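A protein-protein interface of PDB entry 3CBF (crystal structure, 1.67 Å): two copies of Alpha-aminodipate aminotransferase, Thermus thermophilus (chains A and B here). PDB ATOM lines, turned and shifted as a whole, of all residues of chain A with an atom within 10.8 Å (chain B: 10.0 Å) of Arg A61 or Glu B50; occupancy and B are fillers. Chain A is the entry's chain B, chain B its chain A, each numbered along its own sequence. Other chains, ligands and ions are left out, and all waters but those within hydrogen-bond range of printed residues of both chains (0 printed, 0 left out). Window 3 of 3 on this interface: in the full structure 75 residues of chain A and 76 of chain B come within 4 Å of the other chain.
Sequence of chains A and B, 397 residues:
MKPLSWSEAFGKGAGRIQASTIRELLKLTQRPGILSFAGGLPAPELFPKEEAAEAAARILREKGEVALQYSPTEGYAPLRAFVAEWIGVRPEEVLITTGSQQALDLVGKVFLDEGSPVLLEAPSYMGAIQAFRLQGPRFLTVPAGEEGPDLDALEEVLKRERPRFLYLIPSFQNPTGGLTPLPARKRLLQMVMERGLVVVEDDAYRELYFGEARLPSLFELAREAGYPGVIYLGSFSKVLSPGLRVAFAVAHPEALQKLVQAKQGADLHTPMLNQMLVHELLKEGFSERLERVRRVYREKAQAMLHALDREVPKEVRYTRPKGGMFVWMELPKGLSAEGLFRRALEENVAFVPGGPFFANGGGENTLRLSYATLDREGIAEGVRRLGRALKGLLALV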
ATOM      1  N   ALA A  52      13.577  15.770  25.703  1.00  0.00           N
ATOM      2  CA  ALA A  52      13.572  15.464  24.269  1.00  0.00           C
ATOM      3  C   ALA A  52      14.378  14.211  23.967  1.00  0.00           C
ATOM      4  O   ALA A  52      13.960  13.394  23.148  1.00  0.00           O
ATOM      5  CB  ALA A  52      14.116  16.647  23.438  1.00  0.00           C
ATOM      6  N   ALA A  53      15.537  14.067  24.618  1.00  0.00           N
ATOM      7  CA  ALA A  53      16.354  12.865  24.498  1.00  0.00           C
ATOM      8  C   ALA A  53      15.590  11.591  24.873  1.00  0.00           C
ATOM      9  O   ALA A  53      15.618  10.602  24.132  1.00  0.00           O
ATOM     10  CB  ALA A  53      17.646  12.995  25.329  1.00  0.00           C
ATOM     11  N   GLU A  54      14.872  11.626  26.000  1.00  0.00           N
ATOM     12  CA  GLU A  54      14.126  10.453  26.470  1.00  0.00           C
ATOM     13  C   GLU A  54      13.016  10.111  25.485  1.00  0.00           C
ATOM     14  O   GLU A  54      12.784   8.941  25.136  1.00  0.00           O
ATOM     15  CB  GLU A  54      13.541  10.727  27.863  1.00  0.00           C
ATOM     16  CG  GLU A  54      12.828   9.527  28.538  1.00  0.00           C
ATOM     17  CD  GLU A  54      11.406   9.257  28.015  1.00  0.00           C
ATOM     18  OE1 GLU A  54      10.962   8.086  28.073  1.00  0.00           O
ATOM     19  OE2 GLU A  54      10.724  10.205  27.560  1.00  0.00           O
ATOM     20  N   ALA A  55      12.340  11.155  25.024  1.00  0.00           N
ATOM     21  CA  ALA A  55      11.245  11.016  24.069  1.00  0.00           C
ATOM     22  C   ALA A  55      11.686  10.548  22.695  1.00  0.00           C
ATOM     23  O   ALA A  55      11.021   9.700  22.094  1.00  0.00           O
ATOM     24  CB  ALA A  55      10.430  12.308  23.988  1.00  0.00           C
ATOM     25  N   ALA A  56      12.800  11.075  22.206  1.00  0.00           N
ATOM     26  CA  ALA A  56      13.307  10.687  20.875  1.00  0.00           C
ATOM     27  C   ALA A  56      13.664   9.198  20.900  1.00  0.00           C
ATOM     28  O   ALA A  56      13.316   8.460  19.982  1.00  0.00           O
ATOM     29  CB  ALA A  56      14.530  11.530  20.472  1.00  0.00           C
ATOM     30  N   ALA A  57      14.348   8.765  21.959  1.00  0.00           N
ATOM     31  CA  ALA A  57      14.736   7.344  22.078  1.00  0.00           C
ATOM     32  C   ALA A  57      13.532   6.410  22.095  1.00  0.00           C
ATOM     33  O   ALA A  57      13.530   5.374  21.426  1.00  0.00           O
ATOM     34  CB  ALA A  57      15.589   7.124  23.296  1.00  0.00           C
ATOM     35  N   ARG A  58      12.499   6.809  22.831  1.00  0.00           N
ATOM     36  CA  ARG A  58      11.251   6.051  22.949  1.00  0.00           C
ATOM     37  C   ARG A  58      10.527   5.995  21.614  1.00  0.00           C
ATOM     38  O   ARG A  58      10.067   4.941  21.196  1.00  0.00           O
ATOM     39  CB  ARG A  58      10.381   6.683  24.039  1.00  0.00           C
ATOM     40  CG  ARG A  58       9.114   5.940  24.393  1.00  0.00           C
ATOM     41  CD  ARG A  58       8.621   6.347  25.788  1.00  0.00           C
ATOM     42  NE  ARG A  58       8.802   7.771  26.085  1.00  0.00           N
ATOM     43  CZ  ARG A  58       7.916   8.722  25.811  1.00  0.00           C
ATOM     44  NH1 ARG A  58       6.758   8.415  25.228  1.00  0.00           N
ATOM     45  NH2 ARG A  58       8.185   9.982  26.135  1.00  0.00           N
ATOM     46  N   ILE A  59      10.460   7.124  20.916  1.00  0.00           N
ATOM     47  CA  ILE A  59       9.801   7.121  19.616  1.00  0.00           C
ATOM     48  C   ILE A  59      10.519   6.134  18.693  1.00  0.00           C
ATOM     49  O   ILE A  59       9.875   5.342  17.998  1.00  0.00           O
ATOM     50  CB  ILE A  59       9.761   8.544  19.012  1.00  0.00           C
ATOM     51  CG1 ILE A  59       8.741   9.415  19.774  1.00  0.00           C
ATOM     52  CG2 ILE A  59       9.466   8.496  17.504  1.00  0.00           C
ATOM     53  CD1 ILE A  59       8.950  10.949  19.534  1.00  0.00           C
ATOM     54  N   LEU A  60      11.850   6.186  18.680  1.00  0.00           N
ATOM     55  CA  LEU A  60      12.610   5.399  17.711  1.00  0.00           C
ATOM     56  C   LEU A  60      12.580   3.906  18.050  1.00  0.00           C
ATOM     57  O   LEU A  60      12.514   3.067  17.162  1.00  0.00           O
ATOM     58  CB  LEU A  60      14.019   5.945  17.499  1.00  0.00           C
ATOM     59  CG  LEU A  60      14.069   7.323  16.805  1.00  0.00           C
ATOM     60  CD1 LEU A  60      15.346   8.091  17.106  1.00  0.00           C
ATOM     61  CD2 LEU A  60      13.855   7.167  15.295  1.00  0.00           C
ATOM     62  N   ARG A  61      12.575   3.590  19.346  1.00  0.00           N
ATOM     63  CA  ARG A  61      12.433   2.192  19.780  1.00  0.00           C
ATOM     64  C   ARG A  61      11.040   1.615  19.555  1.00  0.00           C
ATOM     65  O   ARG A  61      10.905   0.497  19.030  1.00  0.00           O
ATOM     66  CB  ARG A  61      12.839   2.014  21.243  1.00  0.00           C
ATOM     67  CG  ARG A  61      14.327   2.029  21.436  1.00  0.00           C
ATOM     68  CD  ARG A  61      14.732   1.702  22.874  1.00  0.00           C
ATOM     69  NE  ARG A  61      16.187   1.705  23.015  1.00  0.00           N
ATOM     70  CZ  ARG A  61      16.900   2.701  23.542  1.00  0.00           C
ATOM     71  NH1 ARG A  61      16.301   3.781  24.021  1.00  0.00           N
ATOM     72  NH2 ARG A  61      18.226   2.605  23.611  1.00  0.00           N
ATOM     73  N   GLU A  62      10.011   2.374  19.922  1.00  0.00           N
ATOM     74  CA  GLU A  62       8.627   1.888  19.891  1.00  0.00           C
ATOM     75  C   GLU A  62       7.908   2.110  18.560  1.00  0.00           C
ATOM     76  O   GLU A  62       6.983   1.365  18.213  1.00  0.00           O
ATOM     77  CB  GLU A  62       7.814   2.486  21.053  1.00  0.00           C
ATOM     78  CG  GLU A  62       8.456   2.234  22.439  1.00  0.00           C
ATOM     79  CD  GLU A  62       7.666   2.799  23.618  1.00  0.00           C
ATOM     80  OE1 GLU A  62       8.212   2.787  24.747  1.00  0.00           O
ATOM     81  OE2 GLU A  62       6.513   3.261  23.437  1.00  0.00           O
ATOM     82  N   LYS A  63       8.333   3.131  17.817  1.00  0.00           N
ATOM     83  CA  LYS A  63       7.660   3.524  16.583  1.00  0.00           C
ATOM     84  C   LYS A  63       8.635   3.912  15.477  1.00  0.00           C
ATOM     85  O   LYS A  63       8.264   4.664  14.576  1.00  0.00           O
ATOM     86  CB  LYS A  63       6.712   4.706  16.845  1.00  0.00           C
ATOM     87  CG  LYS A  63       5.676   4.474  17.931  1.00  0.00           C
ATOM     88  CD  LYS A  63       4.819   5.705  18.160  1.00  0.00           C
ATOM     89  CE  LYS A  63       3.653   5.390  19.117  1.00  0.00           C
ATOM     90  NZ  LYS A  63       2.813   6.584  19.422  1.00  0.00           N
ATOM     91  N   GLY A  64       9.865   3.405  15.538  1.00  0.00           N
ATOM     92  CA  GLY A  64      10.910   3.722  14.554  1.00  0.00           C
ATOM     93  C   GLY A  64      10.547   3.501  13.090  1.00  0.00           C
ATOM     94  O   GLY A  64      10.985   4.254  12.206  1.00  0.00           O
ATOM     95  N   GLU A  65       9.743   2.470  12.828  1.00  0.00           N
ATOM     96  CA  GLU A  65       9.324   2.121  11.468  1.00  0.00           C
ATOM     97  C   GLU A  65       8.378   3.173  10.894  1.00  0.00           C
ATOM     98  O   GLU A  65       8.177   3.243   9.685  1.00  0.00           O
ATOM     99  CB  GLU A  65       8.674   0.722  11.427  1.00  0.00           C
ATOM    100  CG  GLU A  65       7.311   0.617  12.124  1.00  0.00           C
ATOM    101  CD  GLU A  65       7.381   0.732  13.660  1.00  0.00           C
ATOM    102  OE1 GLU A  65       6.360   1.161  14.244  1.00  0.00           O
ATOM    103  OE2 GLU A  65       8.439   0.423  14.267  1.00  0.00           O
ATOM    104  N   VAL A  66       7.776   3.962  11.779  1.00  0.00           N
ATOM    105  CA  VAL A  66       6.969   5.106  11.348  1.00  0.00           C
ATOM    106  C   VAL A  66       7.846   6.362  11.281  1.00  0.00           C
ATOM    107  O   VAL A  66       7.799   7.102  10.296  1.00  0.00           O
ATOM    108  CB  VAL A  66       5.732   5.325  12.241  1.00  0.00           C
ATOM    109  CG1 VAL A  66       4.994   6.617  11.826  1.00  0.00           C
ATOM    110  CG2 VAL A  66       4.785   4.130  12.136  1.00  0.00           C
ATOM    111  N   ALA A  67       8.662   6.578  12.308  1.00  0.00           N
ATOM    112  CA  ALA A  67       9.478   7.796  12.414  1.00  0.00           C
ATOM    113  C   ALA A  67      10.471   7.900  11.271  1.00  0.00           C
ATOM    114  O   ALA A  67      10.811   8.998  10.829  1.00  0.00           O
ATOM    115  CB  ALA A  67      10.220   7.826  13.737  1.00  0.00           C
ATOM    116  N   LEU A  68      10.937   6.753  10.792  1.00  0.00           N
ATOM    117  CA  LEU A  68      12.030   6.723   9.831  1.00  0.00           C
ATOM    118  C   LEU A  68      11.582   6.552   8.379  1.00  0.00           C
ATOM    119  O   LEU A  68      12.404   6.630   7.467  1.00  0.00           O
ATOM    120  CB  LEU A  68      13.054   5.642  10.234  1.00  0.00           C
ATOM    121  CG  LEU A  68      13.751   5.918  11.568  1.00  0.00           C
ATOM    122  CD1 LEU A  68      14.576   4.693  12.023  1.00  0.00           C
ATOM    123  CD2 LEU A  68      14.611   7.175  11.548  1.00  0.00           C
ATOM    124  N   LEU A 273      10.068  11.959  12.648  1.00  0.00           N
ATOM    125  CA  LEU A 273      10.671  11.984  13.981  1.00  0.00           C
ATOM    126  C   LEU A 273      10.412  13.315  14.712  1.00  0.00           C
ATOM    127  O   LEU A 273      10.022  13.328  15.891  1.00  0.00           O
ATOM    128  CB  LEU A 273      12.168  11.692  13.904  1.00  0.00           C
ATOM    129  CG  LEU A 273      13.020  11.859  15.176  1.00  0.00           C
ATOM    130  CD1 LEU A 273      12.544  10.947  16.347  1.00  0.00           C
ATOM    131  CD2 LEU A 273      14.469  11.572  14.826  1.00  0.00           C
ATOM    132  N   MET A 276       6.688  13.859  15.605  1.00  0.00           N
ATOM    133  CA  MET A 276       6.353  12.959  16.726  1.00  0.00           C
ATOM    134  C   MET A 276       6.973  13.459  18.041  1.00  0.00           C
ATOM    135  O   MET A 276       6.350  13.393  19.115  1.00  0.00           O
ATOM    136  CB  MET A 276       6.816  11.524  16.400  1.00  0.00           C
ATOM    137  CG  MET A 276       6.105  10.900  15.221  1.00  0.00           C
ATOM    138  SD  MET A 276       6.832   9.362  14.640  1.00  0.00           S
ATOM    139  CE  MET A 276       6.212   8.232  15.879  1.00  0.00           C
ATOM    140  N   GLU A 280       5.087  14.441  21.433  1.00  0.00           N
ATOM    141  CA  GLU A 280       5.418  13.793  22.710  1.00  0.00           C
ATOM    142  C   GLU A 280       5.790  14.796  23.795  1.00  0.00           C
ATOM    143  O   GLU A 280       5.395  14.641  24.946  1.00  0.00           O
ATOM    144  CB  GLU A 280       6.525  12.740  22.554  1.00  0.00           C
ATOM    145  CG  GLU A 280       6.111  11.501  21.736  1.00  0.00           C
ATOM    146  CD  GLU A 280       5.046  10.633  22.406  1.00  0.00           C
ATOM    147  OE1 GLU A 280       5.038  10.542  23.654  1.00  0.00           O
ATOM    148  OE2 GLU A 280       4.229  10.038  21.668  1.00  0.00           O
ATOM    149  N   PRO B  44      11.553  -1.751   5.749  1.00  0.00           N
ATOM    150  CA  PRO B  44      11.511  -1.364   7.166  1.00  0.00           C
ATOM    151  C   PRO B  44      12.536  -2.073   8.061  1.00  0.00           C
ATOM    152  O   PRO B  44      12.965  -1.505   9.064  1.00  0.00           O
ATOM    153  CB  PRO B  44      10.086  -1.735   7.594  1.00  0.00           C
ATOM    154  CG  PRO B  44       9.303  -1.785   6.337  1.00  0.00           C
ATOM    155  CD  PRO B  44      10.243  -2.229   5.271  1.00  0.00           C
ATOM    156  N   GLU B  45      12.934  -3.292   7.717  1.00  0.00           N
ATOM    157  CA  GLU B  45      13.875  -4.013   8.574  1.00  0.00           C
ATOM    158  C   GLU B  45      15.293  -3.520   8.327  1.00  0.00           C
ATOM    159  O   GLU B  45      16.207  -3.868   9.063  1.00  0.00           O
ATOM    160  CB  GLU B  45      13.763  -5.540   8.388  1.00  0.00           C
ATOM    161  CG  GLU B  45      14.711  -6.162   7.368  1.00  0.00           C
ATOM    162  CD  GLU B  45      14.428  -5.719   5.952  1.00  0.00           C
ATOM    163  OE1 GLU B  45      15.324  -5.093   5.338  1.00  0.00           O
ATOM    164  OE2 GLU B  45      13.308  -5.981   5.457  1.00  0.00           O
ATOM    165  N   LEU B  46      15.471  -2.701   7.290  1.00  0.00           N
ATOM    166  CA  LEU B  46      16.757  -2.059   7.034  1.00  0.00           C
ATOM    167  C   LEU B  46      16.958  -0.850   7.949  1.00  0.00           C
ATOM    168  O   LEU B  46      18.074  -0.342   8.033  1.00  0.00           O
ATOM    169  CB  LEU B  46      16.852  -1.642   5.559  1.00  0.00           C
ATOM    170  CG  LEU B  46      18.054  -2.051   4.703  1.00  0.00           C
ATOM    171  CD1 LEU B  46      18.682  -3.371   5.127  1.00  0.00           C
ATOM    172  CD2 LEU B  46      17.673  -2.092   3.225  1.00  0.00           C
ATOM    173  N   PHE B  47      15.878  -0.394   8.610  1.00  0.00           N
ATOM    174  CA  PHE B  47      15.938   0.750   9.534  1.00  0.00           C
ATOM    175  C   PHE B  47      16.630   0.333  10.827  1.00  0.00           C
ATOM    176  O   PHE B  47      16.168  -0.601  11.479  1.00  0.00           O
ATOM    177  CB  PHE B  47      14.541   1.332   9.875  1.00  0.00           C
ATOM    178  CG  PHE B  47      13.808   1.956   8.698  1.00  0.00           C
ATOM    179  CD1 PHE B  47      14.502   2.607   7.684  1.00  0.00           C
ATOM    180  CD2 PHE B  47      12.409   1.929   8.636  1.00  0.00           C
ATOM    181  CE1 PHE B  47      13.824   3.179   6.607  1.00  0.00           C
ATOM    182  CE2 PHE B  47      11.718   2.513   7.570  1.00  0.00           C
ATOM    183  CZ  PHE B  47      12.425   3.134   6.548  1.00  0.00           C
ATOM    184  N   PRO B  48      17.727   1.021  11.189  1.00  0.00           N
ATOM    185  CA  PRO B  48      18.467   0.746  12.418  1.00  0.00           C
ATOM    186  C   PRO B  48      17.843   1.461  13.621  1.00  0.00           C
ATOM    187  O   PRO B  48      18.451   2.387  14.191  1.00  0.00           O
ATOM    188  CB  PRO B  48      19.863   1.289  12.112  1.00  0.00           C
ATOM    189  CG  PRO B  48      19.587   2.470  11.192  1.00  0.00           C
ATOM    190  CD  PRO B  48      18.357   2.097  10.392  1.00  0.00           C
ATOM    191  N   LYS B  49      16.651   1.002  13.996  1.00  0.00           N
ATOM    192  CA  LYS B  49      15.815   1.618  15.034  1.00  0.00           C
ATOM    193  C   LYS B  49      16.523   1.782  16.363  1.00  0.00           C
ATOM    194  O   LYS B  49      16.516   2.870  16.946  1.00  0.00           O
ATOM    195  CB  LYS B  49      14.516   0.814  15.233  1.00  0.00           C
ATOM    196  CG  LYS B  49      13.609   0.779  14.012  1.00  0.00           C
ATOM    197  CD  LYS B  49      12.269   0.089  14.302  1.00  0.00           C
ATOM    198  CE  LYS B  49      12.354  -1.443  14.235  1.00  0.00           C
ATOM    199  NZ  LYS B  49      11.045  -2.056  14.594  1.00  0.00           N
ATOM    200  N   GLU B  50      17.122   0.698  16.858  1.00  0.00           N
ATOM    201  CA  GLU B  50      17.812   0.741  18.144  1.00  0.00           C
ATOM    202  C   GLU B  50      19.036   1.663  18.131  1.00  0.00           C
ATOM    203  O   GLU B  50      19.228   2.456  19.062  1.00  0.00           O
ATOM    204  CB  GLU B  50      18.177  -0.679  18.601  1.00  0.00           C
ATOM    205  CG  GLU B  50      18.756  -0.777  20.007  1.00  0.00           C
ATOM    206  CD  GLU B  50      17.884  -0.111  21.071  1.00  0.00           C
ATOM    207  OE1 GLU B  50      16.803  -0.654  21.406  1.00  0.00           O
ATOM    208  OE2 GLU B  50      18.294   0.958  21.585  1.00  0.00           O
ATOM    209  N   GLU B  51      19.854   1.572  17.082  1.00  0.00           N
ATOM    210  CA  GLU B  51      21.035   2.428  16.979  1.00  0.00           C
ATOM    211  C   GLU B  51      20.636   3.904  16.834  1.00  0.00           C
ATOM    212  O   GLU B  51      21.279   4.775  17.407  1.00  0.00           O
ATOM    213  CB  GLU B  51      21.961   1.980  15.842  1.00  0.00           C
ATOM    214  CG  GLU B  51      23.324   2.685  15.848  1.00  0.00           C
ATOM    215  CD  GLU B  51      24.247   2.278  14.698  1.00  0.00           C
ATOM    216  OE1 GLU B  51      23.850   1.396  13.902  1.00  0.00           O
ATOM    217  OE2 GLU B  51      25.372   2.847  14.596  1.00  0.00           O
ATOM    218  N   ALA B  52      19.558   4.163  16.097  1.00  0.00           N
ATOM    219  CA  ALA B  52      19.030   5.527  15.950  1.00  0.00           C
ATOM    220  C   ALA B  52      18.573   6.064  17.298  1.00  0.00           C
ATOM    221  O   ALA B  52      18.865   7.199  17.644  1.00  0.00           O
ATOM    222  CB  ALA B  52      17.892   5.562  14.940  1.00  0.00           C
ATOM    223  N   ALA B  53      17.883   5.233  18.073  1.00  0.00           N
ATOM    224  CA  ALA B  53      17.366   5.661  19.372  1.00  0.00           C
ATOM    225  C   ALA B  53      18.527   6.095  20.293  1.00  0.00           C
ATOM    226  O   ALA B  53      18.472   7.169  20.908  1.00  0.00           O
ATOM    227  CB  ALA B  53      16.521   4.532  19.998  1.00  0.00           C
ATOM    228  N   GLU B  54      19.568   5.264  20.378  1.00  0.00           N
ATOM    229  CA  GLU B  54      20.755   5.584  21.180  1.00  0.00           C
ATOM    230  C   GLU B  54      21.428   6.865  20.694  1.00  0.00           C
ATOM    231  O   GLU B  54      21.740   7.732  21.525  1.00  0.00           O
ATOM    232  CB  GLU B  54      21.746   4.407  21.185  1.00  0.00           C
ATOM    233  CG  GLU B  54      23.013   4.583  22.052  1.00  0.00           C
ATOM    234  CD  GLU B  54      24.145   5.442  21.449  1.00  0.00           C
ATOM    235  OE1 GLU B  54      24.901   6.036  22.245  1.00  0.00           O
ATOM    236  OE2 GLU B  54      24.299   5.548  20.203  1.00  0.00           O
ATOM    237  N   ALA B  55      21.612   6.992  19.365  1.00  0.00           N
ATOM    238  CA  ALA B  55      22.289   8.153  18.788  1.00  0.00           C
ATOM    239  C   ALA B  55      21.489   9.440  18.950  1.00  0.00           C
ATOM    240  O   ALA B  55      22.062  10.463  19.333  1.00  0.00           O
ATOM    241  CB  ALA B  55      22.676   7.918  17.306  1.00  0.00           C
ATOM    242  N   ALA B  56      20.180   9.387  18.714  1.00  0.00           N
ATOM    243  CA  ALA B  56      19.320  10.571  18.906  1.00  0.00           C
ATOM    244  C   ALA B  56      19.353  11.074  20.333  1.00  0.00           C
ATOM    245  O   ALA B  56      19.502  12.271  20.574  1.00  0.00           O
ATOM    246  CB  ALA B  56      17.858  10.292  18.479  1.00  0.00           C
ATOM    247  N   ALA B  57      19.211  10.132  21.275  1.00  0.00           N
ATOM    248  CA  ALA B  57      19.230  10.443  22.707  1.00  0.00           C
ATOM    249  C   ALA B  57      20.551  11.090  23.115  1.00  0.00           C
ATOM    250  O   ALA B  57      20.547  12.093  23.822  1.00  0.00           O
ATOM    251  CB  ALA B  57      18.962   9.185  23.543  1.00  0.00           C
ATOM    252  N   ARG B  58      21.672  10.547  22.630  1.00  0.00           N
ATOM    253  CA  ARG B  58      22.989  11.079  22.980  1.00  0.00           C
ATOM    254  C   ARG B  58      23.190  12.473  22.352  1.00  0.00           C
ATOM    255  O   ARG B  58      23.677  13.403  22.993  1.00  0.00           O
ATOM    256  CB  ARG B  58      24.089  10.108  22.548  1.00  0.00           C
ATOM    257  CG  ARG B  58      25.453  10.465  23.085  1.00  0.00           C
ATOM    258  CD  ARG B  58      26.618   9.691  22.430  1.00  0.00           C
ATOM    259  NE  ARG B  58      26.225   8.581  21.558  1.00  0.00           N
ATOM    260  CZ  ARG B  58      26.436   8.561  20.243  1.00  0.00           C
ATOM    261  NH1 ARG B  58      27.051   9.584  19.650  1.00  0.00           N
ATOM    262  NH2 ARG B  58      26.055   7.519  19.517  1.00  0.00           N
ATOM    263  N   ARG B  61      21.045  14.913  24.518  1.00  0.00           N
ATOM    264  CA  ARG B  61      21.650  15.093  25.850  1.00  0.00           C
ATOM    265  C   ARG B  61      22.915  15.935  25.805  1.00  0.00           C
ATOM    266  O   ARG B  61      23.023  16.935  26.515  1.00  0.00           O
ATOM    267  CB  ARG B  61      21.970  13.745  26.483  1.00  0.00           C
ATOM    268  CG  ARG B  61      20.772  13.115  27.032  1.00  0.00           C
ATOM    269  CD  ARG B  61      21.035  11.739  27.493  1.00  0.00           C
ATOM    270  NE  ARG B  61      19.711  11.212  27.688  1.00  0.00           N
ATOM    271  CZ  ARG B  61      19.279  10.048  27.245  1.00  0.00           C
ATOM    272  NH1 ARG B  61      20.117   9.194  26.639  1.00  0.00           N
ATOM    273  NH2 ARG B  61      18.016   9.732  27.482  1.00  0.00           N
ATOM    274  N   LEU B 277      22.130  13.141  13.493  1.00  0.00           N
ATOM    275  CA  LEU B 277      21.727  11.734  13.607  1.00  0.00           C
ATOM    276  C   LEU B 277      22.227  10.917  12.414  1.00  0.00           C
ATOM    277  O   LEU B 277      22.798   9.860  12.582  1.00  0.00           O
ATOM    278  CB  LEU B 277      20.202  11.619  13.791  1.00  0.00           C
ATOM    279  CG  LEU B 277      19.600  10.216  13.930  1.00  0.00           C
ATOM    280  CD1 LEU B 277      20.174   9.512  15.188  1.00  0.00           C
ATOM    281  CD2 LEU B 277      18.083  10.278  13.966  1.00  0.00           C
ATOM    282  N   LEU B 281      25.092   7.953  12.762  1.00  0.00           N
ATOM    283  CA  LEU B 281      24.756   6.597  12.321  1.00  0.00           C
ATOM    284  C   LEU B 281      25.722   6.047  11.280  1.00  0.00           C
ATOM    285  O   LEU B 281      25.869   4.832  11.135  1.00  0.00           O
ATOM    286  CB  LEU B 281      23.329   6.559  11.779  1.00  0.00           C
ATOM    287  CG  LEU B 281      22.204   6.598  12.821  1.00  0.00           C
ATOM    288  CD1 LEU B 281      20.860   6.724  12.104  1.00  0.00           C
ATOM    289  CD2 LEU B 281      22.212   5.365  13.707  1.00  0.00           C
ATOM    290  N   ARG B 289      27.297  -1.211   5.918  1.00  0.00           N
ATOM    291  CA  ARG B 289      25.859  -0.948   5.767  1.00  0.00           C
ATOM    292  C   ARG B 289      25.452  -0.948   4.290  1.00  0.00           C
ATOM    293  O   ARG B 289      24.439  -1.539   3.920  1.00  0.00           O
ATOM    294  CB  ARG B 289      25.470   0.388   6.415  1.00  0.00           C
ATOM    295  CG  ARG B 289      24.027   0.781   6.151  1.00  0.00           C
ATOM    296  CD  ARG B 289      23.595   2.053   6.877  1.00  0.00           C
ATOM    297  NE  ARG B 289      23.634   1.872   8.329  1.00  0.00           N
ATOM    298  CZ  ARG B 289      22.672   1.292   9.049  1.00  0.00           C
ATOM    299  NH1 ARG B 289      21.561   0.836   8.470  1.00  0.00           N
ATOM    300  NH2 ARG B 289      22.826   1.170  10.361  1.00  0.00           N
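The side-chain carboxylate (OE2) of Glu A54 lies within salt-bridge range of the guanidinium group (NH2) of Arg A58 (2.9 Å). The backbone carbonyl oxygen (O) of Ile A59 lies within hydrogen-bond range of the backbone NH (N) of Gly A64 (3.1 Å).
Hydrophobic or aromatic side chains of chain B that line the printed part of chain A: Phe B47, Ala B53, Ala B56, Ala B57 and Leu B277. Along chain B the printed residues that touch a printed residue of chain A span positions 47 to 277. Hydrophobic or aromatic side chains of chain A within 4 Å of the printed part of chain B: Ala A53, Ala A57, Leu A60, Leu A68 and Leu A273. Among the printed residues, Asp or Glu carboxylates within 4 Å of a Lys or Arg side-chain nitrogen of the other chain: Arg A61 with Glu B50 (2.6 Å) and Glu A65 with Lys B49 (3.6 Å).
The side-chain amino group (NZ) of Lys B49 is in salt-bridge range of the side-chain carboxylate (OE2) of Glu A65 (3.6 Å). OE2 of Glu B50 is in salt-bridge range of NH2 of Arg A61, 2.6 Å away.
Ala A53 touches Ala B57, and with the chains exchanged Ala A57 touches Ala B53. Ala A53 touches Arg B61, and with the chains exchanged Arg A61 touches Ala B53. Glu A54 touches Arg B61, but with the chains exchanged Arg A61 does not touch Glu B54 (4.4 Å). Ala B57 touches its own counterpart, Ala A57. Positions printed for both chains: 52, 53, 54, 55, 56, 57, 58 and 61.
Of chain B, only Glu B50 and Ala B53 come within 4 Å of Arg A61. Of chain A, only Arg A61 comes within 4 Å of Glu B50. Of chain B, only Ala B53 and Ala B57 come within 4 Å of Ala A57. Leu A60 touches just these residues of chain B: Lys B49 (3.6 Å), Ala B52 (3.7 Å), Ala B53 (3.8 Å) and Ala B56 (3.6 Å). Printed residues of chain A within 4 Å of Ala B52: Leu A60. Of chain A, only Ala A57 (3.4 Å), Leu A60 (3.8 Å) and Arg A61 (3.6 Å) come within 4 Å of Ala B53. Of the printed residues of chain A, Ala B56 touches Leu A60. Of the printed residues of chain B, Glu A54 touches Arg B61. Of the printed residues of chain A, Ala B57 touches Ala A53 (3.4 Å) and Ala A57 (3.96 Å). Printed residues of chain A within 4 Å of Leu B277: Leu A273 (3.9 Å). Printed residues of chain B within 4 Å of Ala A53: Ala B57 (3.4 Å) and Arg B61 (3.6 Å). Leu B281 touches none of the printed residues of chain A. The nearest printed residue of chain A that does not touch Ala B56 is Ala A56 (4.1 Å).
Ala A53 touches Arg B61. Arg B61 touches Glu A54 (NH2 to N, 3.96 Å). Ala A57 touches Ala B53. Ala A57 touches Ala B57 (CB to CB, 3.96 Å). Leu A60 touches Lys B49 (O to CB, 3.6 Å). Leu A60 touches Ala B52. Leu A60 touches Ala B53 (CB to CB, 3.8 Å). CD1 of Leu A60 touches CB of Ala B56, at 3.6 Å. Ala B53 touches Arg A61. Gly A64 touches Lys B49 (CA to CD, 3.9 Å).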
